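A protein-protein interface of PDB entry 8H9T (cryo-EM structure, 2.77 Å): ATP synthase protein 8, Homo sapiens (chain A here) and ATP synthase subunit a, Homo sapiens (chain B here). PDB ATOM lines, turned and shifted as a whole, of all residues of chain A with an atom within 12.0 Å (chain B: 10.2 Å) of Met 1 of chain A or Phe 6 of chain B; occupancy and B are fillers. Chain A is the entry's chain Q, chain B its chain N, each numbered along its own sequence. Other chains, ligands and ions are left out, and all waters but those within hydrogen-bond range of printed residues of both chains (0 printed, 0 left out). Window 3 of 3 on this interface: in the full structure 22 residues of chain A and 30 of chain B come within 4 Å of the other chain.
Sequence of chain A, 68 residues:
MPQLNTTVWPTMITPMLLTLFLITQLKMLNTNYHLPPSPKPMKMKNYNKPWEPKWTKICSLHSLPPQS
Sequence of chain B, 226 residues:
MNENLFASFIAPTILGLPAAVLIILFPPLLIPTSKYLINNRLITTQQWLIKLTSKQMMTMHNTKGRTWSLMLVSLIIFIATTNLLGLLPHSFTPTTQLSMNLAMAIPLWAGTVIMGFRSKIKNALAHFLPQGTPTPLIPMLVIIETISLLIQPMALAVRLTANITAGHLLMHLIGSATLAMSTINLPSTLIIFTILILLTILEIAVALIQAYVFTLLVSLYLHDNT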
ATOM      1  N   MET A   1     -23.838 -13.277   7.365  1.00  0.00           N
ATOM      2  CA  MET A   1     -24.578 -13.944   6.306  1.00  0.00           C
ATOM      3  C   MET A   1     -26.046 -14.045   6.655  1.00  0.00           C
ATOM      4  O   MET A   1     -26.398 -14.460   7.756  1.00  0.00           O
ATOM      5  CB  MET A   1     -24.018 -15.341   6.049  1.00  0.00           C
ATOM      6  CG  MET A   1     -22.639 -15.348   5.448  1.00  0.00           C
ATOM      7  SD  MET A   1     -22.426 -13.993   4.290  1.00  0.00           S
ATOM      8  CE  MET A   1     -22.668 -14.835   2.736  1.00  0.00           C
ATOM      9  N   PRO A   2     -26.909 -13.654   5.718  1.00  0.00           N
ATOM     10  CA  PRO A   2     -28.337 -13.922   5.887  1.00  0.00           C
ATOM     11  C   PRO A   2     -28.713 -15.353   5.562  1.00  0.00           C
ATOM     12  O   PRO A   2     -29.751 -15.823   6.044  1.00  0.00           O
ATOM     13  CB  PRO A   2     -28.991 -12.942   4.913  1.00  0.00           C
ATOM     14  CG  PRO A   2     -27.979 -12.763   3.858  1.00  0.00           C
ATOM     15  CD  PRO A   2     -26.639 -12.853   4.516  1.00  0.00           C
ATOM     16  N   GLN A   3     -27.894 -16.066   4.785  1.00  0.00           N
ATOM     17  CA  GLN A   3     -28.146 -17.469   4.478  1.00  0.00           C
ATOM     18  C   GLN A   3     -28.258 -18.335   5.718  1.00  0.00           C
ATOM     19  O   GLN A   3     -28.646 -19.499   5.598  1.00  0.00           O
ATOM     20  CB  GLN A   3     -27.031 -18.036   3.602  1.00  0.00           C
ATOM     21  CG  GLN A   3     -27.127 -17.702   2.139  1.00  0.00           C
ATOM     22  CD  GLN A   3     -26.649 -16.308   1.832  1.00  0.00           C
ATOM     23  OE1 GLN A   3     -26.428 -15.509   2.734  1.00  0.00           O
ATOM     24  NE2 GLN A   3     -26.477 -16.009   0.555  1.00  0.00           N
ATOM     25  N   LEU A   4     -27.916 -17.818   6.890  1.00  0.00           N
ATOM     26  CA  LEU A   4     -27.908 -18.613   8.103  1.00  0.00           C
ATOM     27  C   LEU A   4     -28.970 -18.191   9.102  1.00  0.00           C
ATOM     28  O   LEU A   4     -28.936 -18.647  10.248  1.00  0.00           O
ATOM     29  CB  LEU A   4     -26.529 -18.560   8.763  1.00  0.00           C
ATOM     30  CG  LEU A   4     -25.461 -19.470   8.161  1.00  0.00           C
ATOM     31  CD1 LEU A   4     -24.944 -18.931   6.852  1.00  0.00           C
ATOM     32  CD2 LEU A   4     -24.321 -19.650   9.128  1.00  0.00           C
ATOM     33  N   ASN A   5     -29.909 -17.335   8.710  1.00  0.00           N
ATOM     34  CA  ASN A   5     -31.028 -16.978   9.578  1.00  0.00           C
ATOM     35  C   ASN A   5     -32.009 -18.144   9.565  1.00  0.00           C
ATOM     36  O   ASN A   5     -33.011 -18.153   8.848  1.00  0.00           O
ATOM     37  CB  ASN A   5     -31.681 -15.686   9.113  1.00  0.00           C
ATOM     38  CG  ASN A   5     -32.971 -15.393   9.840  1.00  0.00           C
ATOM     39  OD1 ASN A   5     -33.145 -15.772  10.995  1.00  0.00           O
ATOM     40  ND2 ASN A   5     -33.889 -14.720   9.163  1.00  0.00           N
ATOM     41  N   THR A   6     -31.724 -19.146  10.389  1.00  0.00           N
ATOM     42  CA  THR A   6     -32.478 -20.387  10.303  1.00  0.00           C
ATOM     43  C   THR A   6     -33.830 -20.269  10.989  1.00  0.00           C
ATOM     44  O   THR A   6     -34.185 -21.098  11.830  1.00  0.00           O
ATOM     45  CB  THR A   6     -31.687 -21.538  10.912  1.00  0.00           C
ATOM     46  OG1 THR A   6     -31.643 -21.383  12.333  1.00  0.00           O
ATOM     47  CG2 THR A   6     -30.281 -21.541  10.379  1.00  0.00           C
ATOM     48  N   THR A   7     -34.584 -19.237  10.635  1.00  0.00           N
ATOM     49  CA  THR A   7     -36.001 -19.156  10.938  1.00  0.00           C
ATOM     50  C   THR A   7     -36.806 -18.897   9.683  1.00  0.00           C
ATOM     51  O   THR A   7     -38.038 -18.828   9.744  1.00  0.00           O
ATOM     52  CB  THR A   7     -36.283 -18.054  11.966  1.00  0.00           C
ATOM     53  OG1 THR A   7     -37.572 -18.271  12.554  1.00  0.00           O
ATOM     54  CG2 THR A   7     -36.264 -16.690  11.298  1.00  0.00           C
ATOM     55  N   VAL A   8     -36.137 -18.750   8.549  1.00  0.00           N
ATOM     56  CA  VAL A   8     -36.756 -18.495   7.263  1.00  0.00           C
ATOM     57  C   VAL A   8     -36.483 -19.646   6.302  1.00  0.00           C
ATOM     58  O   VAL A   8     -36.712 -19.535   5.110  1.00  0.00           O
ATOM     59  CB  VAL A   8     -36.271 -17.148   6.697  1.00  0.00           C
ATOM     60  CG1 VAL A   8     -34.863 -17.276   6.135  1.00  0.00           C
ATOM     61  CG2 VAL A   8     -37.240 -16.599   5.675  1.00  0.00           C
ATOM     62  N   TRP A   9     -36.001 -20.762   6.823  1.00  0.00           N
ATOM     63  CA  TRP A   9     -35.613 -21.869   5.965  1.00  0.00           C
ATOM     64  C   TRP A   9     -36.818 -22.608   5.391  1.00  0.00           C
ATOM     65  O   TRP A   9     -36.836 -22.867   4.184  1.00  0.00           O
ATOM     66  CB  TRP A   9     -34.690 -22.825   6.720  1.00  0.00           C
ATOM     67  CG  TRP A   9     -33.283 -22.355   6.691  1.00  0.00           C
ATOM     68  CD1 TRP A   9     -32.865 -21.085   6.472  1.00  0.00           C
ATOM     69  CD2 TRP A   9     -32.102 -23.143   6.869  1.00  0.00           C
ATOM     70  NE1 TRP A   9     -31.499 -21.027   6.497  1.00  0.00           N
ATOM     71  CE2 TRP A   9     -31.006 -22.279   6.746  1.00  0.00           C
ATOM     72  CE3 TRP A   9     -31.865 -24.493   7.121  1.00  0.00           C
ATOM     73  CZ2 TRP A   9     -29.697 -22.717   6.867  1.00  0.00           C
ATOM     74  CZ3 TRP A   9     -30.563 -24.925   7.242  1.00  0.00           C
ATOM     75  CH2 TRP A   9     -29.498 -24.042   7.115  1.00  0.00           C
ATOM     76  N   MET A  12     -38.222 -21.217   2.266  1.00  0.00           N
ATOM     77  CA  MET A  12     -37.389 -21.412   1.090  1.00  0.00           C
ATOM     78  C   MET A  12     -37.395 -22.854   0.622  1.00  0.00           C
ATOM     79  O   MET A  12     -37.304 -23.105  -0.581  1.00  0.00           O
ATOM     80  CB  MET A  12     -35.946 -20.991   1.368  1.00  0.00           C
ATOM     81  CG  MET A  12     -35.775 -19.541   1.719  1.00  0.00           C
ATOM     82  SD  MET A  12     -36.028 -18.458   0.318  1.00  0.00           S
ATOM     83  CE  MET A  12     -36.080 -16.882   1.155  1.00  0.00           C
ATOM     84  N   ASN B   4     -26.477  -4.260   4.830  1.00  0.00           N
ATOM     85  CA  ASN B   4     -26.326  -3.146   3.903  1.00  0.00           C
ATOM     86  C   ASN B   4     -25.714  -3.615   2.590  1.00  0.00           C
ATOM     87  O   ASN B   4     -25.842  -2.957   1.560  1.00  0.00           O
ATOM     88  CB  ASN B   4     -25.462  -2.045   4.521  1.00  0.00           C
ATOM     89  CG  ASN B   4     -24.084  -2.538   4.913  1.00  0.00           C
ATOM     90  OD1 ASN B   4     -23.935  -3.637   5.445  1.00  0.00           O
ATOM     91  ND2 ASN B   4     -23.066  -1.728   4.647  1.00  0.00           N
ATOM     92  N   LEU B   5     -25.050  -4.761   2.636  1.00  0.00           N
ATOM     93  CA  LEU B   5     -24.400  -5.345   1.473  1.00  0.00           C
ATOM     94  C   LEU B   5     -24.991  -6.681   1.071  1.00  0.00           C
ATOM     95  O   LEU B   5     -25.174  -6.937  -0.119  1.00  0.00           O
ATOM     96  CB  LEU B   5     -22.904  -5.521   1.736  1.00  0.00           C
ATOM     97  CG  LEU B   5     -22.085  -5.976   0.535  1.00  0.00           C
ATOM     98  CD1 LEU B   5     -22.425  -5.134  -0.675  1.00  0.00           C
ATOM     99  CD2 LEU B   5     -20.616  -5.885   0.841  1.00  0.00           C
ATOM    100  N   PHE B   6     -25.289  -7.544   2.031  1.00  0.00           N
ATOM    101  CA  PHE B   6     -25.966  -8.798   1.753  1.00  0.00           C
ATOM    102  C   PHE B   6     -27.463  -8.630   1.596  1.00  0.00           C
ATOM    103  O   PHE B   6     -28.189  -9.626   1.642  1.00  0.00           O
ATOM    104  CB  PHE B   6     -25.680  -9.799   2.865  1.00  0.00           C
ATOM    105  CG  PHE B   6     -24.246 -10.169   2.978  1.00  0.00           C
ATOM    106  CD1 PHE B   6     -23.497  -9.758   4.057  1.00  0.00           C
ATOM    107  CD2 PHE B   6     -23.640 -10.924   1.998  1.00  0.00           C
ATOM    108  CE1 PHE B   6     -22.173 -10.098   4.157  1.00  0.00           C
ATOM    109  CE2 PHE B   6     -22.319 -11.269   2.094  1.00  0.00           C
ATOM    110  CZ  PHE B   6     -21.582 -10.854   3.174  1.00  0.00           C
ATOM    111  N   ALA B   7     -27.940  -7.398   1.420  1.00  0.00           N
ATOM    112  CA  ALA B   7     -29.373  -7.165   1.321  1.00  0.00           C
ATOM    113  C   ALA B   7     -29.997  -7.969   0.195  1.00  0.00           C
ATOM    114  O   ALA B   7     -31.117  -8.467   0.339  1.00  0.00           O
ATOM    115  CB  ALA B   7     -29.649  -5.679   1.118  1.00  0.00           C
ATOM    116  N   SER B   8     -29.292  -8.123  -0.923  1.00  0.00           N
ATOM    117  CA  SER B   8     -29.861  -8.850  -2.047  1.00  0.00           C
ATOM    118  C   SER B   8     -30.070 -10.325  -1.739  1.00  0.00           C
ATOM    119  O   SER B   8     -30.786 -11.001  -2.479  1.00  0.00           O
ATOM    120  CB  SER B   8     -28.970  -8.695  -3.274  1.00  0.00           C
ATOM    121  OG  SER B   8     -27.914  -9.635  -3.248  1.00  0.00           O
ATOM    122  N   PHE B   9     -29.467 -10.841  -0.675  1.00  0.00           N
ATOM    123  CA  PHE B   9     -29.679 -12.222  -0.273  1.00  0.00           C
ATOM    124  C   PHE B   9     -30.587 -12.344   0.938  1.00  0.00           C
ATOM    125  O   PHE B   9     -30.912 -13.464   1.343  1.00  0.00           O
ATOM    126  CB  PHE B   9     -28.339 -12.903   0.008  1.00  0.00           C
ATOM    127  CG  PHE B   9     -27.273 -12.551  -0.977  1.00  0.00           C
ATOM    128  CD1 PHE B   9     -26.153 -11.861  -0.584  1.00  0.00           C
ATOM    129  CD2 PHE B   9     -27.397 -12.901  -2.300  1.00  0.00           C
ATOM    130  CE1 PHE B   9     -25.179 -11.533  -1.488  1.00  0.00           C
ATOM    131  CE2 PHE B   9     -26.422 -12.573  -3.206  1.00  0.00           C
ATOM    132  CZ  PHE B   9     -25.316 -11.889  -2.798  1.00  0.00           C
ATOM    133  N   ILE B  10     -30.996 -11.225   1.532  1.00  0.00           N
ATOM    134  CA  ILE B  10     -31.955 -11.263   2.623  1.00  0.00           C
ATOM    135  C   ILE B  10     -33.284 -11.774   2.096  1.00  0.00           C
ATOM    136  O   ILE B  10     -33.743 -11.362   1.022  1.00  0.00           O
ATOM    137  CB  ILE B  10     -32.104  -9.868   3.249  1.00  0.00           C
ATOM    138  CG1 ILE B  10     -30.879  -9.533   4.097  1.00  0.00           C
ATOM    139  CG2 ILE B  10     -33.369  -9.781   4.072  1.00  0.00           C
ATOM    140  CD1 ILE B  10     -30.930  -8.163   4.721  1.00  0.00           C
ATOM    141  N   ALA B  11     -33.898 -12.687   2.839  1.00  0.00           N
ATOM    142  CA  ALA B  11     -35.180 -13.259   2.464  1.00  0.00           C
ATOM    143  C   ALA B  11     -36.170 -12.153   2.108  1.00  0.00           C
ATOM    144  O   ALA B  11     -36.389 -11.243   2.919  1.00  0.00           O
ATOM    145  CB  ALA B  11     -35.732 -14.109   3.601  1.00  0.00           C
ATOM    146  N   PRO B  12     -36.767 -12.186   0.925  1.00  0.00           N
ATOM    147  CA  PRO B  12     -37.597 -11.069   0.484  1.00  0.00           C
ATOM    148  C   PRO B  12     -38.968 -11.096   1.127  1.00  0.00           C
ATOM    149  O   PRO B  12     -39.428 -12.113   1.644  1.00  0.00           O
ATOM    150  CB  PRO B  12     -37.705 -11.298  -1.022  1.00  0.00           C
ATOM    151  CG  PRO B  12     -37.656 -12.755  -1.147  1.00  0.00           C
ATOM    152  CD  PRO B  12     -36.726 -13.258  -0.077  1.00  0.00           C
ATOM    153  N   SER B  91     -33.028  -8.535  -8.278  1.00  0.00           N
ATOM    154  CA  SER B  91     -33.704  -9.821  -8.286  1.00  0.00           C
ATOM    155  C   SER B  91     -33.111 -10.739  -7.233  1.00  0.00           C
ATOM    156  O   SER B  91     -31.891 -10.838  -7.101  1.00  0.00           O
ATOM    157  CB  SER B  91     -33.606 -10.466  -9.655  1.00  0.00           C
ATOM    158  OG  SER B  91     -34.233  -9.648 -10.620  1.00  0.00           O
ATOM    159  N   PHE B  92     -33.979 -11.415  -6.492  1.00  0.00           N
ATOM    160  CA  PHE B  92     -33.564 -12.313  -5.423  1.00  0.00           C
ATOM    161  C   PHE B  92     -33.386 -13.712  -5.992  1.00  0.00           C
ATOM    162  O   PHE B  92     -34.369 -14.390  -6.298  1.00  0.00           O
ATOM    163  CB  PHE B  92     -34.594 -12.318  -4.302  1.00  0.00           C
ATOM    164  CG  PHE B  92     -34.473 -13.486  -3.381  1.00  0.00           C
ATOM    165  CD1 PHE B  92     -33.390 -13.611  -2.549  1.00  0.00           C
ATOM    166  CD2 PHE B  92     -35.443 -14.454  -3.345  1.00  0.00           C
ATOM    167  CE1 PHE B  92     -33.278 -14.679  -1.704  1.00  0.00           C
ATOM    168  CE2 PHE B  92     -35.333 -15.523  -2.499  1.00  0.00           C
ATOM    169  CZ  PHE B  92     -34.251 -15.635  -1.679  1.00  0.00           C
ATOM    170  N   THR B  93     -32.138 -14.152  -6.118  1.00  0.00           N
ATOM    171  CA  THR B  93     -31.838 -15.454  -6.693  1.00  0.00           C
ATOM    172  C   THR B  93     -31.960 -16.538  -5.640  1.00  0.00           C
ATOM    173  O   THR B  93     -31.097 -16.638  -4.764  1.00  0.00           O
ATOM    174  CB  THR B  93     -30.427 -15.486  -7.257  1.00  0.00           C
ATOM    175  OG1 THR B  93     -30.245 -14.385  -8.145  1.00  0.00           O
ATOM    176  CG2 THR B  93     -30.215 -16.757  -8.014  1.00  0.00           C
ATOM    177  N   THR B  96     -28.893 -18.682  -4.314  1.00  0.00           N
ATOM    178  CA  THR B  96     -27.905 -18.166  -3.382  1.00  0.00           C
ATOM    179  C   THR B  96     -28.162 -18.619  -1.962  1.00  0.00           C
ATOM    180  O   THR B  96     -27.257 -18.520  -1.130  1.00  0.00           O
ATOM    181  CB  THR B  96     -27.879 -16.649  -3.404  1.00  0.00           C
ATOM    182  OG1 THR B  96     -29.017 -16.154  -2.698  1.00  0.00           O
ATOM    183  CG2 THR B  96     -27.921 -16.146  -4.813  1.00  0.00           C
ATOM    184  N   GLN B  97     -29.360 -19.097  -1.659  1.00  0.00           N
ATOM    185  CA  GLN B  97     -29.660 -19.567  -0.319  1.00  0.00           C
ATOM    186  C   GLN B  97     -29.067 -20.947  -0.099  1.00  0.00           C
ATOM    187  O   GLN B  97     -29.096 -21.799  -0.986  1.00  0.00           O
ATOM    188  CB  GLN B  97     -31.165 -19.598  -0.098  1.00  0.00           C
ATOM    189  CG  GLN B  97     -31.821 -18.269  -0.339  1.00  0.00           C
ATOM    190  CD  GLN B  97     -31.489 -17.273   0.735  1.00  0.00           C
ATOM    191  OE1 GLN B  97     -31.431 -17.615   1.910  1.00  0.00           O
ATOM    192  NE2 GLN B  97     -31.267 -16.031   0.345  1.00  0.00           N
ATOM    193  N   LEU B  98     -28.505 -21.158   1.084  1.00  0.00           N
ATOM    194  CA  LEU B  98     -27.995 -22.475   1.420  1.00  0.00           C
ATOM    195  C   LEU B  98     -29.119 -23.459   1.668  1.00  0.00           C
ATOM    196  O   LEU B  98     -28.930 -24.665   1.489  1.00  0.00           O
ATOM    197  CB  LEU B  98     -27.104 -22.388   2.651  1.00  0.00           C
ATOM    198  CG  LEU B  98     -26.294 -23.631   2.974  1.00  0.00           C
ATOM    199  CD1 LEU B  98     -25.574 -24.089   1.742  1.00  0.00           C
ATOM    200  CD2 LEU B  98     -25.315 -23.313   4.068  1.00  0.00           C
ATOM    201  N   THR B 161     -23.968 -22.804  -3.956  1.00  0.00           N
ATOM    202  CA  THR B 161     -24.352 -21.680  -3.118  1.00  0.00           C
ATOM    203  C   THR B 161     -23.338 -20.559  -3.200  1.00  0.00           C
ATOM    204  O   THR B 161     -23.696 -19.382  -3.122  1.00  0.00           O
ATOM    205  CB  THR B 161     -24.503 -22.144  -1.677  1.00  0.00           C
ATOM    206  OG1 THR B 161     -25.583 -23.075  -1.596  1.00  0.00           O
ATOM    207  CG2 THR B 161     -24.780 -20.975  -0.765  1.00  0.00           C
ATOM    208  N   ALA B 162     -22.066 -20.901  -3.384  1.00  0.00           N
ATOM    209  CA  ALA B 162     -21.043 -19.871  -3.481  1.00  0.00           C
ATOM    210  C   ALA B 162     -20.991 -19.284  -4.872  1.00  0.00           C
ATOM    211  O   ALA B 162     -21.051 -18.061  -5.043  1.00  0.00           O
ATOM    212  CB  ALA B 162     -19.679 -20.437  -3.130  1.00  0.00           C
ATOM    213  N   ILE B 164     -22.780 -18.821  -7.223  1.00  0.00           N
ATOM    214  CA  ILE B 164     -23.749 -17.776  -7.488  1.00  0.00           C
ATOM    215  C   ILE B 164     -23.545 -16.603  -6.545  1.00  0.00           C
ATOM    216  O   ILE B 164     -23.230 -15.495  -6.988  1.00  0.00           O
ATOM    217  CB  ILE B 164     -25.174 -18.344  -7.383  1.00  0.00           C
ATOM    218  CG1 ILE B 164     -25.289 -19.602  -8.227  1.00  0.00           C
ATOM    219  CG2 ILE B 164     -26.178 -17.333  -7.859  1.00  0.00           C
ATOM    220  CD1 ILE B 164     -25.036 -19.357  -9.669  1.00  0.00           C
ATOM    221  N   THR B 165     -23.670 -16.855  -5.238  1.00  0.00           N
ATOM    222  CA  THR B 165     -23.533 -15.807  -4.232  1.00  0.00           C
ATOM    223  C   THR B 165     -22.332 -14.926  -4.513  1.00  0.00           C
ATOM    224  O   THR B 165     -22.473 -13.739  -4.828  1.00  0.00           O
ATOM    225  CB  THR B 165     -23.380 -16.418  -2.848  1.00  0.00           C
ATOM    226  OG1 THR B 165     -24.508 -17.243  -2.559  1.00  0.00           O
ATOM    227  CG2 THR B 165     -23.277 -15.334  -1.816  1.00  0.00           C
ATOM    228  N   ALA B 166     -21.139 -15.514  -4.441  1.00  0.00           N
ATOM    229  CA  ALA B 166     -19.919 -14.787  -4.745  1.00  0.00           C
ATOM    230  C   ALA B 166     -20.093 -13.994  -6.025  1.00  0.00           C
ATOM    231  O   ALA B 166     -20.064 -12.759  -6.011  1.00  0.00           O
ATOM    232  CB  ALA B 166     -18.741 -15.755  -4.851  1.00  0.00           C
ATOM    233  N   GLY B 167     -20.366 -14.697  -7.118  1.00  0.00           N
ATOM    234  CA  GLY B 167     -20.553 -14.068  -8.405  1.00  0.00           C
ATOM    235  C   GLY B 167     -21.400 -12.826  -8.293  1.00  0.00           C
ATOM    236  O   GLY B 167     -20.968 -11.736  -8.677  1.00  0.00           O
ATOM    237  N   HIS B 168     -22.577 -12.961  -7.689  1.00  0.00           N
ATOM    238  CA  HIS B 168     -23.467 -11.816  -7.587  1.00  0.00           C
ATOM    239  C   HIS B 168     -22.793 -10.669  -6.856  1.00  0.00           C
ATOM    240  O   HIS B 168     -22.640  -9.574  -7.413  1.00  0.00           O
ATOM    241  CB  HIS B 168     -24.764 -12.223  -6.905  1.00  0.00           C
ATOM    242  CG  HIS B 168     -25.750 -12.833  -7.842  1.00  0.00           C
ATOM    243  ND1 HIS B 168     -25.395 -13.793  -8.764  1.00  0.00           N
ATOM    244  CD2 HIS B 168     -27.070 -12.605  -8.026  1.00  0.00           C
ATOM    245  CE1 HIS B 168     -26.458 -14.140  -9.467  1.00  0.00           C
ATOM    246  NE2 HIS B 168     -27.486 -13.433  -9.038  1.00  0.00           N
ATOM    247  N   LEU B 169     -22.351 -10.916  -5.616  1.00  0.00           N
ATOM    248  CA  LEU B 169     -21.618  -9.909  -4.858  1.00  0.00           C
ATOM    249  C   LEU B 169     -20.624  -9.232  -5.761  1.00  0.00           C
ATOM    250  O   LEU B 169     -20.580  -8.002  -5.863  1.00  0.00           O
ATOM    251  CB  LEU B 169     -20.886 -10.548  -3.680  1.00  0.00           C
ATOM    252  CG  LEU B 169     -21.665 -10.863  -2.413  1.00  0.00           C
ATOM    253  CD1 LEU B 169     -20.848 -11.766  -1.537  1.00  0.00           C
ATOM    254  CD2 LEU B 169     -21.971  -9.580  -1.694  1.00  0.00           C
ATOM    255  N   LEU B 170     -19.862 -10.052  -6.470  1.00  0.00           N
ATOM    256  CA  LEU B 170     -18.806  -9.571  -7.333  1.00  0.00           C
ATOM    257  C   LEU B 170     -19.314  -8.458  -8.234  1.00  0.00           C
ATOM    258  O   LEU B 170     -18.899  -7.303  -8.103  1.00  0.00           O
ATOM    259  CB  LEU B 170     -18.257 -10.768  -8.095  1.00  0.00           C
ATOM    260  CG  LEU B 170     -16.973 -10.627  -8.870  1.00  0.00           C
ATOM    261  CD1 LEU B 170     -16.093 -11.802  -8.641  1.00  0.00           C
ATOM    262  CD2 LEU B 170     -17.331 -10.614 -10.252  1.00  0.00           C
ATOM    263  N   HIS B 172     -22.041  -6.773  -8.092  1.00  0.00           N
ATOM    264  CA  HIS B 172     -22.544  -5.702  -7.247  1.00  0.00           C
ATOM    265  C   HIS B 172     -21.443  -4.710  -6.929  1.00  0.00           C
ATOM    266  O   HIS B 172     -21.589  -3.506  -7.165  1.00  0.00           O
ATOM    267  CB  HIS B 172     -23.127  -6.298  -5.970  1.00  0.00           C
ATOM    268  CG  HIS B 172     -23.825  -5.304  -5.104  1.00  0.00           C
ATOM    269  ND1 HIS B 172     -23.148  -4.404  -4.315  1.00  0.00           N
ATOM    270  CD2 HIS B 172     -25.140  -5.082  -4.886  1.00  0.00           C
ATOM    271  CE1 HIS B 172     -24.016  -3.658  -3.657  1.00  0.00           C
ATOM    272  NE2 HIS B 172     -25.233  -4.050  -3.985  1.00  0.00           N
ATOM    273  N   LEU B 173     -20.294  -5.213  -6.478  1.00  0.00           N
ATOM    274  CA  LEU B 173     -19.266  -4.302  -5.996  1.00  0.00           C
ATOM    275  C   LEU B 173     -18.735  -3.425  -7.117  1.00  0.00           C
ATOM    276  O   LEU B 173     -18.574  -2.215  -6.929  1.00  0.00           O
ATOM    277  CB  LEU B 173     -18.141  -5.074  -5.319  1.00  0.00           C
ATOM    278  CG  LEU B 173     -18.594  -5.620  -3.970  1.00  0.00           C
ATOM    279  CD1 LEU B 173     -17.448  -6.282  -3.268  1.00  0.00           C
ATOM    280  CD2 LEU B 173     -19.186  -4.524  -3.108  1.00  0.00           C
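The side-chain amide nitrogen of Gln 3 of chain A sits at hydrogen-bond distance from the backbone carbonyl oxygen of Thr 96 of chain B (3.1 Å).
O of Gln 3 of chain A is in hydrogen-bond range of NE1 of Trp 9 of chain A, 3.4 Å away.
OG1 of Thr 96 of chain B lies within hydrogen-bond range of O of Thr 93 of chain B, at 3.0 Å.
The side-chain amide nitrogen (NE2) of Gln 97 of chain B sits at hydrogen-bond distance from the backbone carbonyl oxygen (O) of Phe 9 of chain B, 2.8 Å away.
The backbone carbonyl oxygen (O) of Thr 96 of chain B is in hydrogen-bond range of the side-chain hydroxyl (OG1) of Thr 165 of chain B (3.4 Å).
Among the printed residues, pairs that only touch across the chains: Met 1 of chain A with Phe 6 of chain B, Val 8 of chain A with Ala 11 of chain B, Met 12 of chain A with Phe 92 of chain B, Pro 2 of chain A with Phe 6 of chain B, Gln 3 of chain A with Phe 9 of chain B, Met 12 of chain A with Ala 11 of chain B, Gln 3 of chain A with Leu 98 of chain B, Pro 2 of chain A with Phe 9 of chain B, Met 12 of chain A with Pro 12 of chain B, Gln 3 of chain A with Thr 165 of chain B, Pro 2 of chain A with Ile 10 of chain B and Gln 3 of chain A with Gln 97 of chain B.
Of chain B, only Phe 6 comes within 4 Å of Met 1 of chain A.
Printed residues of chain A within 4 Å of Phe 6 of chain B: Met 1 (3.4 Å) and Pro 2 (3.6 Å).
No residue of chain B comes within 4 Å of Leu 4 of chain A.
No residue of chain A comes within 4 Å of Asn 4 of chain B.
No residue of chain A comes within 4 Å of Leu 5 of chain B.
No residue of chain A comes within 4 Å of Ala 7 of chain B.
Of chain A, only Pro 2 and Gln 3 come within 4 Å of Phe 9 of chain B.
Of the printed residues of chain A, Gln 97 of chain B touches Gln 3.
Of the printed residues of chain B, Pro 2 of chain A touches Phe 6 (3.6 Å), Phe 9 (3.9 Å) and Ile 10 (3.98 Å).
Ala 162 of chain B touches none of the printed residues of chain A.
Asn 5 of chain A touches none of the printed residues of chain B.
The nearest residue of chain B that does not touch Met 1 of chain A is Thr 165 of chain B (4.6 Å).
The nearest printed residue of chain A that does not touch Ala 11 of chain B is Pro 2 of chain A (5.3 Å).
Hydrophobic or aromatic side chains of chain B within 4 Å of the printed part of chain A: Phe 6, Phe 9, Ile 10, Ala 11, Pro 12 and Phe 92.
Printed residues of chain A that touch a printed residue of chain B: Met 1, Pro 2, Gln 3, Val 8 and Met 12.
Hydrophobic or aromatic side chains of chain A that line the printed part of chain B: Met 1, Pro 2, Val 8 and Met 12.
Among the printed residues, no Asp or Glu carboxylate lies within 4 Å of a Lys or Arg side-chain nitrogen of the other chain.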
